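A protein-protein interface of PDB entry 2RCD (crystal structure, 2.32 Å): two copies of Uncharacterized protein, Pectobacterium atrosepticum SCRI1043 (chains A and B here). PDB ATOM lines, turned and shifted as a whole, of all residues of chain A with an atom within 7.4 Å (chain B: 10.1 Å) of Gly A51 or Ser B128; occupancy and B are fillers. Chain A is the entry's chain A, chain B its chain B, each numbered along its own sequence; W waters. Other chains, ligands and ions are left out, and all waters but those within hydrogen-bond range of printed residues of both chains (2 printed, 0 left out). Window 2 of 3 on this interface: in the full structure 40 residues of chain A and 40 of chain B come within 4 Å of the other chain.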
ATOM      1  N   ARG A  47      30.989 -29.416 -12.292  1.00  0.00           N
ATOM      2  CA  ARG A  47      29.970 -30.419 -12.019  1.00  0.00           C
ATOM      3  C   ARG A  47      28.633 -29.893 -12.500  1.00  0.00           C
ATOM      4  O   ARG A  47      28.141 -28.890 -11.986  1.00  0.00           O
ATOM      5  CB  ARG A  47      29.900 -30.829 -10.542  1.00  0.00           C
ATOM      6  CG  ARG A  47      28.682 -31.676 -10.256  1.00  0.00           C
ATOM      7  CD  ARG A  47      28.595 -32.240  -8.859  1.00  0.00           C
ATOM      8  NE  ARG A  47      27.509 -33.223  -8.812  1.00  0.00           N
ATOM      9  CZ  ARG A  47      26.210 -32.901  -8.781  1.00  0.00           C
ATOM     10  NH1 ARG A  47      25.798 -31.632  -8.829  1.00  0.00           N
ATOM     11  NH2 ARG A  47      25.301 -33.872  -8.758  1.00  0.00           N
ATOM     12  N   TYR A  48      28.096 -30.538 -13.537  1.00  0.00           N
ATOM     13  CA  TYR A  48      26.786 -30.234 -14.070  1.00  0.00           C
ATOM     14  C   TYR A  48      25.872 -31.280 -13.485  1.00  0.00           C
ATOM     15  O   TYR A  48      26.006 -32.454 -13.764  1.00  0.00           O
ATOM     16  CB  TYR A  48      26.761 -30.324 -15.576  1.00  0.00           C
ATOM     17  CG  TYR A  48      27.509 -29.251 -16.316  1.00  0.00           C
ATOM     18  CD1 TYR A  48      27.616 -27.980 -15.815  1.00  0.00           C
ATOM     19  CD2 TYR A  48      28.028 -29.496 -17.584  1.00  0.00           C
ATOM     20  CE1 TYR A  48      28.268 -26.960 -16.526  1.00  0.00           C
ATOM     21  CE2 TYR A  48      28.683 -28.495 -18.300  1.00  0.00           C
ATOM     22  CZ  TYR A  48      28.791 -27.221 -17.753  1.00  0.00           C
ATOM     23  OH  TYR A  48      29.433 -26.211 -18.411  1.00  0.00           O
ATOM     24  N   GLY A  49      24.960 -30.865 -12.628  1.00  0.00           N
ATOM     25  CA  GLY A  49      24.052 -31.798 -11.955  1.00  0.00           C
ATOM     26  C   GLY A  49      22.694 -31.602 -12.572  1.00  0.00           C
ATOM     27  O   GLY A  49      22.545 -30.747 -13.433  1.00  0.00           O
ATOM     28  N   ALA A  50      21.710 -32.370 -12.101  1.00  0.00           N
ATOM     29  CA  ALA A  50      20.348 -32.359 -12.643  1.00  0.00           C
ATOM     30  C   ALA A  50      19.740 -30.969 -12.728  1.00  0.00           C
ATOM     31  O   ALA A  50      19.178 -30.617 -13.751  1.00  0.00           O
ATOM     32  CB  ALA A  50      19.455 -33.275 -11.830  1.00  0.00           C
ATOM     33  N   GLY A  51      19.893 -30.169 -11.684  1.00  0.00           N
ATOM     34  CA  GLY A  51      19.302 -28.838 -11.659  1.00  0.00           C
ATOM     35  C   GLY A  51      20.270 -27.714 -11.384  1.00  0.00           C
ATOM     36  O   GLY A  51      19.844 -26.630 -11.002  1.00  0.00           O
ATOM     37  N   GLU A  52      21.567 -27.952 -11.561  1.00  0.00           N
ATOM     38  CA  GLU A  52      22.535 -26.899 -11.321  1.00  0.00           C
ATOM     39  C   GLU A  52      23.855 -27.109 -12.050  1.00  0.00           C
ATOM     40  O   GLU A  52      24.303 -28.249 -12.269  1.00  0.00           O
ATOM     41  CB  GLU A  52      22.800 -26.714  -9.819  1.00  0.00           C
ATOM     42  CG  GLU A  52      23.335 -27.949  -9.089  1.00  0.00           C
ATOM     43  CD  GLU A  52      22.307 -29.080  -8.936  1.00  0.00           C
ATOM     44  OE1 GLU A  52      21.137 -28.777  -8.594  1.00  0.00           O
ATOM     45  OE2 GLU A  52      22.677 -30.276  -9.117  1.00  0.00           O
ATOM     46  N   ASN A  53      24.475 -25.973 -12.377  1.00  0.00           N
ATOM     47  CA  ASN A  53      25.751 -25.889 -13.071  1.00  0.00           C
ATOM     48  C   ASN A  53      26.759 -25.313 -12.104  1.00  0.00           C
ATOM     49  O   ASN A  53      26.659 -24.133 -11.755  1.00  0.00           O
ATOM     50  CB  ASN A  53      25.604 -24.940 -14.258  1.00  0.00           C
ATOM     51  CG  ASN A  53      24.534 -25.380 -15.203  1.00  0.00           C
ATOM     52  OD1 ASN A  53      24.391 -26.569 -15.463  1.00  0.00           O
ATOM     53  ND2 ASN A  53      23.761 -24.437 -15.708  1.00  0.00           N
ATOM     54  N   PHE A  63      27.059 -26.649  -2.820  1.00  0.00           N
ATOM     55  CA  PHE A  63      26.047 -27.607  -3.328  1.00  0.00           C
ATOM     56  C   PHE A  63      25.866 -28.825  -2.427  1.00  0.00           C
ATOM     57  O   PHE A  63      24.752 -29.160  -2.035  1.00  0.00           O
ATOM     58  CB  PHE A  63      26.374 -28.135  -4.760  1.00  0.00           C
ATOM     59  CG  PHE A  63      25.506 -29.304  -5.171  1.00  0.00           C
ATOM     60  CD1 PHE A  63      24.155 -29.122  -5.440  1.00  0.00           C
ATOM     61  CD2 PHE A  63      26.018 -30.600  -5.221  1.00  0.00           C
ATOM     62  CE1 PHE A  63      23.335 -30.208  -5.778  1.00  0.00           C
ATOM     63  CE2 PHE A  63      25.199 -31.685  -5.551  1.00  0.00           C
ATOM     64  CZ  PHE A  63      23.861 -31.489  -5.823  1.00  0.00           C
ATOM     65  N   VAL A 124      25.698 -34.872 -14.634  1.00  0.00           N
ATOM     66  CA  VAL A 124      24.607 -35.730 -14.181  1.00  0.00           C
ATOM     67  C   VAL A 124      23.325 -35.067 -14.667  1.00  0.00           C
ATOM     68  O   VAL A 124      23.151 -33.850 -14.541  1.00  0.00           O
ATOM     69  CB  VAL A 124      24.584 -35.891 -12.615  1.00  0.00           C
ATOM     70  CG1 VAL A 124      23.420 -36.783 -12.153  1.00  0.00           C
ATOM     71  CG2 VAL A 124      25.923 -36.443 -12.106  1.00  0.00           C
ATOM     72  N   SER A 125      22.435 -35.861 -15.251  1.00  0.00           N
ATOM     73  CA  SER A 125      21.168 -35.333 -15.730  1.00  0.00           C
ATOM     74  C   SER A 125      20.122 -36.424 -15.805  1.00  0.00           C
ATOM     75  O   SER A 125      20.433 -37.612 -15.717  1.00  0.00           O
ATOM     76  CB  SER A 125      21.325 -34.732 -17.127  1.00  0.00           C
ATOM     77  OG  SER A 125      21.601 -35.734 -18.091  1.00  0.00           O
ATOM     78  N   LEU A 126      18.887 -35.982 -16.003  1.00  0.00           N
ATOM     79  CA  LEU A 126      17.757 -36.852 -16.183  1.00  0.00           C
ATOM     80  C   LEU A 126      17.412 -36.773 -17.650  1.00  0.00           C
ATOM     81  O   LEU A 126      17.348 -35.677 -18.218  1.00  0.00           O
ATOM     82  CB  LEU A 126      16.564 -36.358 -15.370  1.00  0.00           C
ATOM     83  CG  LEU A 126      16.670 -36.325 -13.839  1.00  0.00           C
ATOM     84  CD1 LEU A 126      15.391 -35.714 -13.252  1.00  0.00           C
ATOM     85  CD2 LEU A 126      16.931 -37.726 -13.268  1.00  0.00           C
ATOM     86  N   ALA B  50      20.314 -35.310 -24.782  1.00  0.00           N
ATOM     87  CA  ALA B  50      19.083 -34.839 -24.095  1.00  0.00           C
ATOM     88  C   ALA B  50      17.997 -35.905 -23.886  1.00  0.00           C
ATOM     89  O   ALA B  50      17.422 -35.997 -22.820  1.00  0.00           O
ATOM     90  CB  ALA B  50      18.493 -33.649 -24.854  1.00  0.00           C
ATOM     91  N   GLU B  94      27.943 -24.422 -21.321  1.00  0.00           N
ATOM     92  CA  GLU B  94      26.496 -24.328 -21.284  1.00  0.00           C
ATOM     93  C   GLU B  94      26.108 -23.750 -22.653  1.00  0.00           C
ATOM     94  O   GLU B  94      26.952 -23.234 -23.394  1.00  0.00           O
ATOM     95  CB  GLU B  94      25.984 -23.398 -20.192  1.00  0.00           C
ATOM     96  CG  GLU B  94      26.272 -23.809 -18.776  1.00  0.00           C
ATOM     97  CD  GLU B  94      26.094 -22.651 -17.774  1.00  0.00           C
ATOM     98  OE1 GLU B  94      25.516 -21.597 -18.127  1.00  0.00           O
ATOM     99  OE2 GLU B  94      26.552 -22.776 -16.621  1.00  0.00           O
ATOM    100  N   THR B 101      13.688 -21.887 -23.281  1.00  0.00           N
ATOM    101  CA  THR B 101      13.915 -21.227 -21.993  1.00  0.00           C
ATOM    102  C   THR B 101      14.891 -22.035 -21.138  1.00  0.00           C
ATOM    103  O   THR B 101      15.489 -21.499 -20.205  1.00  0.00           O
ATOM    104  CB  THR B 101      12.614 -21.168 -21.189  1.00  0.00           C
ATOM    105  OG1 THR B 101      11.512 -21.031 -22.093  1.00  0.00           O
ATOM    106  CG2 THR B 101      12.647 -20.015 -20.161  1.00  0.00           C
ATOM    107  N   LYS B 102      15.010 -23.329 -21.448  1.00  0.00           N
ATOM    108  CA  LYS B 102      15.854 -24.250 -20.714  1.00  0.00           C
ATOM    109  C   LYS B 102      17.336 -24.048 -21.078  1.00  0.00           C
ATOM    110  O   LYS B 102      17.649 -23.594 -22.177  1.00  0.00           O
ATOM    111  CB  LYS B 102      15.399 -25.693 -20.992  1.00  0.00           C
ATOM    112  N   ILE B 103      18.223 -24.378 -20.134  1.00  0.00           N
ATOM    113  CA  ILE B 103      19.674 -24.222 -20.274  1.00  0.00           C
ATOM    114  C   ILE B 103      20.299 -25.572 -20.615  1.00  0.00           C
ATOM    115  O   ILE B 103      20.096 -26.554 -19.904  1.00  0.00           O
ATOM    116  CB  ILE B 103      20.308 -23.720 -18.957  1.00  0.00           C
ATOM    117  CG1 ILE B 103      19.584 -22.474 -18.422  1.00  0.00           C
ATOM    118  CG2 ILE B 103      21.785 -23.429 -19.151  1.00  0.00           C
ATOM    119  CD1 ILE B 103      19.713 -21.223 -19.328  1.00  0.00           C
ATOM    120  N   GLY B 104      21.048 -25.622 -21.707  1.00  0.00           N
ATOM    121  CA  GLY B 104      21.698 -26.839 -22.120  1.00  0.00           C
ATOM    122  C   GLY B 104      23.104 -26.910 -21.555  1.00  0.00           C
ATOM    123  O   GLY B 104      23.738 -25.890 -21.257  1.00  0.00           O
ATOM    124  N   ARG B 105      23.581 -28.132 -21.384  1.00  0.00           N
ATOM    125  CA  ARG B 105      24.921 -28.374 -20.914  1.00  0.00           C
ATOM    126  C   ARG B 105      25.551 -29.442 -21.778  1.00  0.00           C
ATOM    127  O   ARG B 105      24.925 -30.467 -22.107  1.00  0.00           O
ATOM    128  CB  ARG B 105      24.938 -28.866 -19.459  1.00  0.00           C
ATOM    129  CG  ARG B 105      24.362 -27.900 -18.417  1.00  0.00           C
ATOM    130  CD  ARG B 105      22.851 -27.980 -18.226  1.00  0.00           C
ATOM    131  NE  ARG B 105      22.462 -29.333 -17.842  1.00  0.00           N
ATOM    132  CZ  ARG B 105      22.612 -29.873 -16.627  1.00  0.00           C
ATOM    133  NH1 ARG B 105      23.163 -29.192 -15.634  1.00  0.00           N
ATOM    134  NH2 ARG B 105      22.208 -31.123 -16.412  1.00  0.00           N
ATOM    135  N   SER B 125      22.629 -32.414 -21.992  1.00  0.00           N
ATOM    136  CA  SER B 125      21.348 -32.484 -21.306  1.00  0.00           C
ATOM    137  C   SER B 125      20.815 -31.116 -21.021  1.00  0.00           C
ATOM    138  O   SER B 125      21.586 -30.138 -21.026  1.00  0.00           O
ATOM    139  CB  SER B 125      21.486 -33.173 -19.946  1.00  0.00           C
ATOM    140  OG  SER B 125      22.092 -32.311 -19.002  1.00  0.00           O
ATOM    141  N   LEU B 126      19.510 -31.064 -20.721  1.00  0.00           N
ATOM    142  CA  LEU B 126      18.862 -29.806 -20.344  1.00  0.00           C
ATOM    143  C   LEU B 126      18.706 -29.784 -18.823  1.00  0.00           C
ATOM    144  O   LEU B 126      18.341 -30.783 -18.186  1.00  0.00           O
ATOM    145  CB  LEU B 126      17.514 -29.630 -21.048  1.00  0.00           C
ATOM    146  CG  LEU B 126      17.568 -29.720 -22.574  1.00  0.00           C
ATOM    147  CD1 LEU B 126      16.164 -29.674 -23.153  1.00  0.00           C
ATOM    148  CD2 LEU B 126      18.442 -28.634 -23.172  1.00  0.00           C
ATOM    149  N   MET B 127      19.016 -28.645 -18.232  1.00  0.00           N
ATOM    150  CA  MET B 127      18.940 -28.533 -16.802  1.00  0.00           C
ATOM    151  C   MET B 127      17.466 -28.534 -16.427  1.00  0.00           C
ATOM    152  O   MET B 127      16.682 -27.753 -16.960  1.00  0.00           O
ATOM    153  CB  MET B 127      19.607 -27.256 -16.357  1.00  0.00           C
ATOM    154  CG  MET B 127      19.902 -27.229 -14.918  1.00  0.00           C
ATOM    155  SD  MET B 127      20.777 -25.579 -14.568  1.00  0.00           S
ATOM    156  CE  MET B 127      19.253 -24.378 -14.330  1.00  0.00           C
ATOM    157  N   SER B 128      17.107 -29.432 -15.517  1.00  0.00           N
ATOM    158  CA  SER B 128      15.735 -29.608 -15.076  1.00  0.00           C
ATOM    159  C   SER B 128      15.296 -28.581 -14.041  1.00  0.00           C
ATOM    160  O   SER B 128      16.121 -27.842 -13.525  1.00  0.00           O
ATOM    161  CB  SER B 128      15.584 -31.012 -14.504  1.00  0.00           C
ATOM    162  OG  SER B 128      16.497 -31.203 -13.447  1.00  0.00           O
HETATM  163  O   HOH W   1      18.521 -33.244 -16.079  1.00  0.00           O
HETATM  164  O   HOH W   2      18.224 -34.045 -20.708  1.00  0.00           O
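The side-chain hydroxyl (OG) of Ser B128 lies within hydrogen-bond range of the backbone carbonyl oxygen (O) of Ala A50, at 2.8 Å.
The backbone carbonyl oxygen (O) of Val A124 sits at hydrogen-bond distance from the guanidinium group (NH2) of Arg B105.
The side-chain amide nitrogen of Asn A53 lies within hydrogen-bond range of the side-chain sulfur of Met B127, at 3.4 Å.
ND2 of Asn A53 lies close to OE2 of Glu B94.
The side-chain amide oxygen (OD1) of Asn A53 is in hydrogen-bond range of the guanidinium group (NH1) of Arg B105, 2.9 Å away.
NH1 of Arg B105 is in hydrogen-bond range of O of Gly A49, at 2.8 Å.
The backbone carbonyl oxygen of Ser B125 is in hydrogen-bond range of the backbone NH of Arg B105, 2.9 Å away.
O of Tyr A48 is in hydrogen-bond range of N of Val A124 (2.6 Å).
The backbone NH of Ala A50 lies within hydrogen-bond range of the backbone carbonyl oxygen of Val A124 (3.2 Å).
OE2 of Glu A52 is in salt-bridge range of NH1 of Arg A47, at 3.4 Å.
O of Ile B103 lies within hydrogen-bond range of N of Met B127, at 2.9 Å.
Tyr A48 touches Glu B94.
Arg B105 touches Tyr A48 (CB to CD2, 3.7 Å).
O of Ala A50 touches CG of Met B127 (3.7 Å).
Gly A51 touches Met B127.
Gly A51 touches Ser B128.
O of Glu A52 touches NH1 of Arg B105 (3.7 Å).
N of Glu A52 touches CG of Met B127, 3.8 Å away.
Ser A125 touches Arg B105.
Ser B125 touches Ser A125 (OG to CB, 3.2 Å).
Of chain B, only Met B127 and Ser B128 come within 4 Å of Gly A51.
Ala A50 touches just these residues of chain B: Met B127 and Ser B128.
Of chain B, only Arg B105 (3.7 Å) and Met B127 (3.8 Å) come within 4 Å of Glu A52.
Printed residues of chain A within 4 Å of Ser B125: Ser A125.
Of the printed residues of chain B, Val A124 touches Arg B105.
Of the printed residues of chain B, Tyr A48 touches Glu B94 and Arg B105.
Printed residues of chain B within 4 Å of Asn A53: Glu B94 (3.3 Å), Arg B105 (2.9 Å) and Met B127 (3.4 Å).
Of the printed residues of chain A, Glu B94 touches Tyr A48 and Asn A53.
Leu A126 touches none of the printed residues of chain B.
Lys B102 touches none of the printed residues of chain A.
Of the 11 printed residues of chain A, 8 touch a printed residue of chain B.
Hydrophobic or aromatic side chains of chain A within 4 Å of the printed part of chain B: Tyr A48 and Ala A50.
Of the 11 printed residues of chain B, 5 touch a printed residue of chain A.
Hydrophobic or aromatic side chains of chain B that line the printed part of chain A: Met B127.
Ser B125 touches its own counterpart, Ser A125.
Positions printed for both chains: 50, 125 and 126.
Of the 15 pairs that touch across the chains among the printed residues, 1 has its exchanged pair printed and touching as well.
Water W1 lies within hydrogen-bond range of the backbone NH of Leu A126 (2.8 Å) and the backbone carbonyl oxygen of Leu B126 (3.2 Å).
Water W2 lies within hydrogen-bond range of O of Ala B50 (3.0 Å), O of Leu A126 (3.1 Å) and N of Leu B126 (3.2 Å).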
